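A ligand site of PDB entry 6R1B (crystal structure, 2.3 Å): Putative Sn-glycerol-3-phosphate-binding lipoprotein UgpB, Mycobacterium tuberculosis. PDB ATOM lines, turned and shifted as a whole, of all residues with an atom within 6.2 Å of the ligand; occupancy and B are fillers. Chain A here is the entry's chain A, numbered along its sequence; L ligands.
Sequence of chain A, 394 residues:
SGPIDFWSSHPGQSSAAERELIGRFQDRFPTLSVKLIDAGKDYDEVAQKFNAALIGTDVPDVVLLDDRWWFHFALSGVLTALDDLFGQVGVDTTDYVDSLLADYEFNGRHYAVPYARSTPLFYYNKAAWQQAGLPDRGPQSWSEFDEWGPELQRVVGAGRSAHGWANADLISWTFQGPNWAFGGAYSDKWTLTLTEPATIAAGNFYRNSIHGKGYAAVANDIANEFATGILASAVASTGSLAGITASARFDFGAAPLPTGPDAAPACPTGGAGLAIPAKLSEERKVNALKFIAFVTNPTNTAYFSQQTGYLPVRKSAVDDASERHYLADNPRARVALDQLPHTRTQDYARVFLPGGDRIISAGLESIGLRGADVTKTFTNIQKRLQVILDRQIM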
ATOM      1  N   SER A   9      -1.060 -27.555  20.110  1.00  0.00           N
ATOM      2  CA  SER A   9       0.005 -28.011  19.230  1.00  0.00           C
ATOM      3  C   SER A   9       1.025 -26.917  18.972  1.00  0.00           C
ATOM      4  O   SER A   9       1.918 -27.091  18.137  1.00  0.00           O
ATOM      5  CB  SER A   9      -0.578 -28.525  17.908  1.00  0.00           C
ATOM      6  OG  SER A   9      -1.280 -27.485  17.244  1.00  0.00           O
ATOM      7  N   PRO A  11       0.663 -24.067  17.341  1.00  0.00           N
ATOM      8  CA  PRO A  11       0.674 -23.784  15.910  1.00  0.00           C
ATOM      9  C   PRO A  11       1.435 -22.508  15.606  1.00  0.00           C
ATOM     10  O   PRO A  11       1.328 -21.514  16.331  1.00  0.00           O
ATOM     11  CB  PRO A  11      -0.817 -23.643  15.564  1.00  0.00           C
ATOM     12  CG  PRO A  11      -1.448 -23.237  16.852  1.00  0.00           C
ATOM     13  CD  PRO A  11      -0.690 -23.976  17.918  1.00  0.00           C
ATOM     14  N   GLY A  12       2.176 -22.529  14.510  1.00  0.00           N
ATOM     15  CA  GLY A  12       3.004 -21.385  14.174  1.00  0.00           C
ATOM     16  C   GLY A  12       4.175 -21.200  15.104  1.00  0.00           C
ATOM     17  O   GLY A  12       4.635 -20.067  15.302  1.00  0.00           O
ATOM     18  N   TYR A  43      -2.388 -30.619  14.434  1.00  0.00           N
ATOM     19  CA  TYR A  43      -3.781 -30.735  14.873  1.00  0.00           C
ATOM     20  C   TYR A  43      -4.239 -32.186  14.951  1.00  0.00           C
ATOM     21  O   TYR A  43      -5.074 -32.527  15.800  1.00  0.00           O
ATOM     22  CB  TYR A  43      -4.684 -29.951  13.915  1.00  0.00           C
ATOM     23  CG  TYR A  43      -4.385 -28.468  13.895  1.00  0.00           C
ATOM     24  CD1 TYR A  43      -4.090 -27.790  15.073  1.00  0.00           C
ATOM     25  CD2 TYR A  43      -4.400 -27.761  12.699  1.00  0.00           C
ATOM     26  CE1 TYR A  43      -3.839 -26.429  15.055  1.00  0.00           C
ATOM     27  CE2 TYR A  43      -4.149 -26.409  12.677  1.00  0.00           C
ATOM     28  CZ  TYR A  43      -3.874 -25.745  13.859  1.00  0.00           C
ATOM     29  OH  TYR A  43      -3.614 -24.396  13.847  1.00  0.00           O
ATOM     30  N   ASP A  66      -8.918 -28.200  15.137  1.00  0.00           N
ATOM     31  CA  ASP A  66      -8.803 -27.478  13.865  1.00  0.00           C
ATOM     32  C   ASP A  66     -10.143 -27.460  13.133  1.00  0.00           C
ATOM     33  O   ASP A  66     -11.177 -27.880  13.648  1.00  0.00           O
ATOM     34  CB  ASP A  66      -7.651 -28.041  13.029  1.00  0.00           C
ATOM     35  CG  ASP A  66      -8.016 -29.291  12.248  1.00  0.00           C
ATOM     36  OD1 ASP A  66      -9.159 -29.789  12.353  1.00  0.00           O
ATOM     37  OD2 ASP A  66      -7.132 -29.786  11.525  1.00  0.00           O
ATOM     38  N   ASP A  67     -10.130 -26.950  11.897  1.00  0.00           N
ATOM     39  CA  ASP A  67     -11.348 -26.725  11.119  1.00  0.00           C
ATOM     40  C   ASP A  67     -12.078 -28.009  10.766  1.00  0.00           C
ATOM     41  O   ASP A  67     -13.191 -27.943  10.230  1.00  0.00           O
ATOM     42  CB  ASP A  67     -11.022 -25.944   9.841  1.00  0.00           C
ATOM     43  CG  ASP A  67      -9.838 -26.545   9.080  1.00  0.00           C
ATOM     44  OD1 ASP A  67      -9.185 -27.435   9.623  1.00  0.00           O
ATOM     45  OD2 ASP A  67      -9.575 -26.100   7.946  1.00  0.00           O
ATOM     46  N   ARG A  68     -11.496 -29.166  11.037  1.00  0.00           N
ATOM     47  CA  ARG A  68     -12.170 -30.425  10.797  1.00  0.00           C
ATOM     48  C   ARG A  68     -12.528 -31.146  12.083  1.00  0.00           C
ATOM     49  O   ARG A  68     -13.608 -31.732  12.174  1.00  0.00           O
ATOM     50  CB  ARG A  68     -11.278 -31.318   9.912  1.00  0.00           C
ATOM     51  CG  ARG A  68     -10.582 -30.495   8.811  1.00  0.00           C
ATOM     52  CD  ARG A  68      -9.364 -31.164   8.266  1.00  0.00           C
ATOM     53  NE  ARG A  68      -8.362 -31.345   9.316  1.00  0.00           N
ATOM     54  CZ  ARG A  68      -7.575 -32.410   9.377  1.00  0.00           C
ATOM     55  NH1 ARG A  68      -7.686 -33.356   8.461  1.00  0.00           N
ATOM     56  NH2 ARG A  68      -6.698 -32.525  10.373  1.00  0.00           N
ATOM     57  N   ALA A 116      -6.292 -19.695  16.482  1.00  0.00           N
ATOM     58  CA  ALA A 116      -5.234 -19.599  15.500  1.00  0.00           C
ATOM     59  C   ALA A 116      -5.920 -19.744  14.146  1.00  0.00           C
ATOM     60  O   ALA A 116      -6.111 -20.852  13.644  1.00  0.00           O
ATOM     61  CB  ALA A 116      -4.165 -20.654  15.726  1.00  0.00           C
ATOM     62  N   ARG A 117      -6.325 -18.607  13.588  1.00  0.00           N
ATOM     63  CA  ARG A 117      -7.100 -18.578  12.355  1.00  0.00           C
ATOM     64  C   ARG A 117      -6.265 -17.981  11.227  1.00  0.00           C
ATOM     65  O   ARG A 117      -5.460 -17.066  11.436  1.00  0.00           O
ATOM     66  CB  ARG A 117      -8.409 -17.799  12.565  1.00  0.00           C
ATOM     67  CG  ARG A 117      -9.299 -18.347  13.726  1.00  0.00           C
ATOM     68  CD  ARG A 117      -9.584 -19.854  13.556  1.00  0.00           C
ATOM     69  NE  ARG A 117     -10.004 -20.111  12.179  1.00  0.00           N
ATOM     70  CZ  ARG A 117     -11.263 -20.101  11.766  1.00  0.00           C
ATOM     71  NH1 ARG A 117     -12.269 -19.908  12.617  1.00  0.00           N
ATOM     72  NH2 ARG A 117     -11.512 -20.305  10.473  1.00  0.00           N
ATOM     73  N   SER A 118      -6.479 -18.482  10.018  1.00  0.00           N
ATOM     74  CA  SER A 118      -5.590 -18.207   8.902  1.00  0.00           C
ATOM     75  C   SER A 118      -6.357 -18.064   7.595  1.00  0.00           C
ATOM     76  O   SER A 118      -7.551 -18.332   7.504  1.00  0.00           O
ATOM     77  CB  SER A 118      -4.583 -19.337   8.748  1.00  0.00           C
ATOM     78  OG  SER A 118      -5.289 -20.550   8.522  1.00  0.00           O
ATOM     79  N   THR A 119      -5.634 -17.624   6.578  1.00  0.00           N
ATOM     80  CA  THR A 119      -5.889 -17.893   5.173  1.00  0.00           C
ATOM     81  C   THR A 119      -4.581 -18.401   4.614  1.00  0.00           C
ATOM     82  O   THR A 119      -3.517 -18.127   5.178  1.00  0.00           O
ATOM     83  CB  THR A 119      -6.336 -16.649   4.381  1.00  0.00           C
ATOM     84  OG1 THR A 119      -5.220 -15.767   4.193  1.00  0.00           O
ATOM     85  CG2 THR A 119      -7.458 -15.880   5.105  1.00  0.00           C
ATOM     86  N   ASP A 169      -0.368 -33.619   4.013  1.00  0.00           N
ATOM     87  CA  ASP A 169      -0.668 -32.971   5.283  1.00  0.00           C
ATOM     88  C   ASP A 169      -1.526 -31.724   5.123  1.00  0.00           C
ATOM     89  O   ASP A 169      -2.177 -31.302   6.081  1.00  0.00           O
ATOM     90  CB  ASP A 169       0.625 -32.620   6.022  1.00  0.00           C
ATOM     91  CG  ASP A 169       1.323 -33.846   6.581  1.00  0.00           C
ATOM     92  OD1 ASP A 169       0.638 -34.779   7.037  1.00  0.00           O
ATOM     93  OD2 ASP A 169       2.577 -33.873   6.556  1.00  0.00           O
ATOM     94  N   LEU A 170      -1.560 -31.138   3.932  1.00  0.00           N
ATOM     95  CA  LEU A 170      -2.241 -29.857   3.795  1.00  0.00           C
ATOM     96  C   LEU A 170      -2.777 -29.597   2.388  1.00  0.00           C
ATOM     97  O   LEU A 170      -3.427 -28.562   2.203  1.00  0.00           O
ATOM     98  CB  LEU A 170      -1.285 -28.731   4.210  1.00  0.00           C
ATOM     99  CG  LEU A 170      -1.943 -27.539   4.882  1.00  0.00           C
ATOM    100  CD1 LEU A 170      -2.966 -28.014   5.884  1.00  0.00           C
ATOM    101  CD2 LEU A 170      -0.882 -26.684   5.551  1.00  0.00           C
ATOM    102  N   TRP A 173      -6.336 -28.417   1.745  1.00  0.00           N
ATOM    103  CA  TRP A 173      -6.631 -27.043   2.141  1.00  0.00           C
ATOM    104  C   TRP A 173      -6.073 -26.035   1.150  1.00  0.00           C
ATOM    105  O   TRP A 173      -6.753 -25.061   0.809  1.00  0.00           O
ATOM    106  CB  TRP A 173      -6.074 -26.787   3.545  1.00  0.00           C
ATOM    107  CG  TRP A 173      -6.429 -25.447   4.104  1.00  0.00           C
ATOM    108  CD1 TRP A 173      -7.677 -24.988   4.436  1.00  0.00           C
ATOM    109  CD2 TRP A 173      -5.513 -24.405   4.450  1.00  0.00           C
ATOM    110  NE1 TRP A 173      -7.592 -23.718   4.944  1.00  0.00           N
ATOM    111  CE2 TRP A 173      -6.272 -23.344   4.973  1.00  0.00           C
ATOM    112  CE3 TRP A 173      -4.115 -24.275   4.373  1.00  0.00           C
ATOM    113  CZ2 TRP A 173      -5.690 -22.148   5.393  1.00  0.00           C
ATOM    114  CZ3 TRP A 173      -3.543 -23.079   4.792  1.00  0.00           C
ATOM    115  CH2 TRP A 173      -4.321 -22.041   5.315  1.00  0.00           C
ATOM    116  N   ALA A 223       6.789 -24.896   4.389  1.00  0.00           N
ATOM    117  CA  ALA A 223       7.246 -23.618   4.912  1.00  0.00           C
ATOM    118  C   ALA A 223       8.764 -23.537   4.927  1.00  0.00           C
ATOM    119  O   ALA A 223       9.354 -22.534   4.497  1.00  0.00           O
ATOM    120  CB  ALA A 223       6.675 -23.390   6.312  1.00  0.00           C
ATOM    121  N   SER A 237       0.194 -21.572   4.925  1.00  0.00           N
ATOM    122  CA  SER A 237      -0.610 -20.782   5.845  1.00  0.00           C
ATOM    123  C   SER A 237       0.108 -19.483   6.213  1.00  0.00           C
ATOM    124  O   SER A 237       1.325 -19.459   6.387  1.00  0.00           O
ATOM    125  CB  SER A 237      -0.915 -21.559   7.117  1.00  0.00           C
ATOM    126  OG  SER A 237      -1.512 -20.693   8.069  1.00  0.00           O
ATOM    127  N   THR A 238      -0.678 -18.422   6.389  1.00  0.00           N
ATOM    128  CA  THR A 238      -0.176 -17.221   7.038  1.00  0.00           C
ATOM    129  C   THR A 238       0.280 -17.508   8.447  1.00  0.00           C
ATOM    130  O   THR A 238       1.020 -16.705   9.026  1.00  0.00           O
ATOM    131  CB  THR A 238      -1.243 -16.134   7.040  1.00  0.00           C
ATOM    132  OG1 THR A 238      -0.693 -14.911   7.553  1.00  0.00           O
ATOM    133  CG2 THR A 238      -2.440 -16.567   7.897  1.00  0.00           C
ATOM    134  N   GLY A 239      -0.165 -18.631   9.020  1.00  0.00           N
ATOM    135  CA  GLY A 239       0.293 -19.025  10.344  1.00  0.00           C
ATOM    136  C   GLY A 239       1.773 -19.349  10.404  1.00  0.00           C
ATOM    137  O   GLY A 239       2.363 -19.326  11.495  1.00  0.00           O
ATOM    138  N   SER A 240       2.393 -19.627   9.260  1.00  0.00           N
ATOM    139  CA  SER A 240       3.826 -19.887   9.199  1.00  0.00           C
ATOM    140  C   SER A 240       4.622 -18.640   8.866  1.00  0.00           C
ATOM    141  O   SER A 240       5.819 -18.740   8.569  1.00  0.00           O
ATOM    142  CB  SER A 240       4.145 -20.974   8.161  1.00  0.00           C
ATOM    143  OG  SER A 240       3.339 -22.126   8.325  1.00  0.00           O
ATOM    144  N   THR A 269     -10.626 -19.840   4.645  1.00  0.00           N
ATOM    145  CA  THR A 269      -9.994 -19.634   5.941  1.00  0.00           C
ATOM    146  C   THR A 269      -9.556 -20.983   6.498  1.00  0.00           C
ATOM    147  O   THR A 269      -9.915 -22.036   5.965  1.00  0.00           O
ATOM    148  CB  THR A 269     -10.945 -18.955   6.931  1.00  0.00           C
ATOM    149  OG1 THR A 269     -12.136 -19.731   7.054  1.00  0.00           O
ATOM    150  CG2 THR A 269     -11.298 -17.536   6.486  1.00  0.00           C
ATOM    151  N   GLY A 270      -8.793 -20.955   7.578  1.00  0.00           N
ATOM    152  CA  GLY A 270      -8.398 -22.188   8.218  1.00  0.00           C
ATOM    153  C   GLY A 270      -7.943 -21.944   9.637  1.00  0.00           C
ATOM    154  O   GLY A 270      -8.214 -20.894  10.213  1.00  0.00           O
ATOM    155  N   GLY A 271      -7.227 -22.928  10.183  1.00  0.00           N
ATOM    156  CA  GLY A 271      -6.742 -22.851  11.541  1.00  0.00           C
ATOM    157  C   GLY A 271      -7.642 -23.549  12.558  1.00  0.00           C
ATOM    158  O   GLY A 271      -8.380 -24.477  12.223  1.00  0.00           O
ATOM    159  N   ALA A 272      -7.593 -23.095  13.805  1.00  0.00           N
ATOM    160  CA  ALA A 272      -8.199 -23.833  14.894  1.00  0.00           C
ATOM    161  C   ALA A 272      -8.797 -22.892  15.930  1.00  0.00           C
ATOM    162  O   ALA A 272      -8.446 -21.703  16.018  1.00  0.00           O
ATOM    163  CB  ALA A 272      -7.166 -24.768  15.562  1.00  0.00           C
ATOM    164  N   TYR A 310      -0.790 -15.457  12.310  1.00  0.00           N
ATOM    165  CA  TYR A 310      -2.210 -15.744  12.346  1.00  0.00           C
ATOM    166  C   TYR A 310      -3.027 -14.438  12.407  1.00  0.00           C
ATOM    167  O   TYR A 310      -2.491 -13.347  12.642  1.00  0.00           O
ATOM    168  CB  TYR A 310      -2.552 -16.638  13.525  1.00  0.00           C
ATOM    169  CG  TYR A 310      -2.283 -18.097  13.266  1.00  0.00           C
ATOM    170  CD1 TYR A 310      -3.041 -18.811  12.331  1.00  0.00           C
ATOM    171  CD2 TYR A 310      -1.277 -18.769  13.944  1.00  0.00           C
ATOM    172  CE1 TYR A 310      -2.804 -20.143  12.073  1.00  0.00           C
ATOM    173  CE2 TYR A 310      -1.030 -20.115  13.693  1.00  0.00           C
ATOM    174  CZ  TYR A 310      -1.799 -20.797  12.759  1.00  0.00           C
ATOM    175  OH  TYR A 310      -1.553 -22.130  12.502  1.00  0.00           O
ATOM    176  N   GLN A 346     -15.564 -23.335   3.672  1.00  0.00           N
ATOM    177  CA  GLN A 346     -14.886 -24.527   3.175  1.00  0.00           C
ATOM    178  C   GLN A 346     -15.885 -25.571   2.678  1.00  0.00           C
ATOM    179  O   GLN A 346     -16.996 -25.704   3.208  1.00  0.00           O
ATOM    180  CB  GLN A 346     -13.983 -25.114   4.262  1.00  0.00           C
ATOM    181  CG  GLN A 346     -12.746 -24.241   4.570  1.00  0.00           C
ATOM    182  CD  GLN A 346     -11.628 -25.016   5.255  1.00  0.00           C
ATOM    183  OE1 GLN A 346     -10.964 -25.847   4.647  1.00  0.00           O
ATOM    184  NE2 GLN A 346     -11.399 -24.724   6.536  1.00  0.00           N
ATOM    185  N   ARG A 350     -14.455 -31.686   2.587  1.00  0.00           N
ATOM    186  CA  ARG A 350     -13.184 -31.639   3.304  1.00  0.00           C
ATOM    187  C   ARG A 350     -13.384 -31.537   4.817  1.00  0.00           C
ATOM    188  O   ARG A 350     -12.760 -32.275   5.577  1.00  0.00           O
ATOM    189  CB  ARG A 350     -12.320 -30.473   2.829  1.00  0.00           C
ATOM    190  CG  ARG A 350     -11.021 -30.363   3.638  1.00  0.00           C
ATOM    191  CD  ARG A 350     -10.060 -29.228   3.206  1.00  0.00           C
ATOM    192  NE  ARG A 350      -8.848 -29.334   4.008  1.00  0.00           N
ATOM    193  CZ  ARG A 350      -8.696 -28.810   5.229  1.00  0.00           C
ATOM    194  NH1 ARG A 350      -9.684 -28.095   5.776  1.00  0.00           N
ATOM    195  NH2 ARG A 350      -7.577 -29.002   5.901  1.00  0.00           N
ATOM    196  N   ASP A 357     -11.616 -35.779   4.332  1.00  0.00           N
ATOM    197  CA  ASP A 357     -10.355 -35.081   4.058  1.00  0.00           C
ATOM    198  C   ASP A 357      -9.212 -36.060   3.838  1.00  0.00           C
ATOM    199  O   ASP A 357      -8.353 -35.850   2.974  1.00  0.00           O
ATOM    200  CB  ASP A 357     -10.038 -34.103   5.183  1.00  0.00           C
ATOM    201  CG  ASP A 357      -8.769 -33.310   4.914  1.00  0.00           C
ATOM    202  OD1 ASP A 357      -7.913 -33.235   5.798  1.00  0.00           O
ATOM    203  OD2 ASP A 357      -8.618 -32.790   3.785  1.00  0.00           O
HETATM  204  C1  LIG L   1      -4.742 -24.957   7.981  1.00  0.00           C
HETATM  205  C2  LIG L   1      -5.919 -25.897   7.859  1.00  0.00           C
HETATM  206  C3  LIG L   1      -5.731 -27.184   8.637  1.00  0.00           C
HETATM  207  C4  LIG L   1      -1.528 -25.619   9.634  1.00  0.00           C
HETATM  208  C5  LIG L   1      -0.047 -25.818   9.419  1.00  0.00           C
HETATM  209  C6  LIG L   1       0.568 -25.320  11.784  1.00  0.00           C
HETATM  210  C7  LIG L   1       0.765 -23.564  10.111  1.00  0.00           C
HETATM  211  C8  LIG L   1       2.286 -25.471  10.063  1.00  0.00           C
HETATM  212  N1  LIG L   1       0.881 -25.040  10.355  1.00  0.00           N
HETATM  213  O1  LIG L   1      -7.123 -25.236   8.285  1.00  0.00           O
HETATM  214  O2  LIG L   1      -6.799 -28.090   8.358  1.00  0.00           O
HETATM  215  O3  LIG L   1      -3.482 -22.333   9.073  1.00  0.00           O
HETATM  216  O4  LIG L   1      -3.249 -23.527  11.346  1.00  0.00           O
HETATM  217  O5  LIG L   1      -4.434 -24.677   9.365  1.00  0.00           O
HETATM  218  O6  LIG L   1      -1.893 -24.262   9.294  1.00  0.00           O
HETATM  219  P1  LIG L   1      -3.308 -23.612   9.798  1.00  0.00           P
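NH1 of Arg 350 lies within hydrogen-bond range of OE1 of Gln 346 (2.8 Å). The side-chain carboxylate of Asp 67 lies within hydrogen-bond range of the side-chain amide nitrogen of Gln 346 (2.7 Å). The side-chain hydroxyl of Ser 237 is in hydrogen-bond range of the backbone NH of Gly 239, 2.6 Å away. The backbone carbonyl oxygen (O) of Ser 118 sits at hydrogen-bond distance from the backbone NH (N) of Gly 270 (2.9 Å). The side-chain carboxylate of Asp 67 lies within salt-bridge range of the guanidinium group of Arg 350. The backbone carbonyl oxygen (O) of Gly 271 lies within hydrogen-bond range of the backbone NH (N) of Asp 67. The side-chain hydroxyl (OG) of Ser 118 is in hydrogen-bond range of the backbone NH (N) of Gly 271 (3.5 Å). The side-chain hydroxyl (OH) of Tyr 310 sits at hydrogen-bond distance from the side-chain hydroxyl (OH) of Tyr 43, at 3.3 Å.
Residues that only touch the ligand: Gly 270, Ser 240, Asp 66, Trp 173, Arg 68 and Leu 170. Hydrophobic or aromatic side chains that line the ligand: Tyr 43, Leu 170, Trp 173 and Tyr 310.
An oxygen (O1) of the ligand lies within hydrogen-bond range of the backbone NH (N) of Gly 271, at 3.0 Å. NH2 of Arg 350 is in hydrogen-bond range of O2 of the ligand, 2.7 Å away. OD2 of Asp 67 is in hydrogen-bond range of O1 of the ligand (2.6 Å). O4 of the ligand sits at hydrogen-bond distance from OH of Tyr 310, at 2.5 Å. O3 of the ligand sits at hydrogen-bond distance from OG of Ser 237 (2.8 Å). The side-chain hydroxyl of Tyr 43 lies within hydrogen-bond range of an oxygen (O4) of the ligand, 2.7 Å away. An oxygen (O3) of the ligand lies within hydrogen-bond range of the side-chain hydroxyl (OG) of Ser 118, 2.6 Å away.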
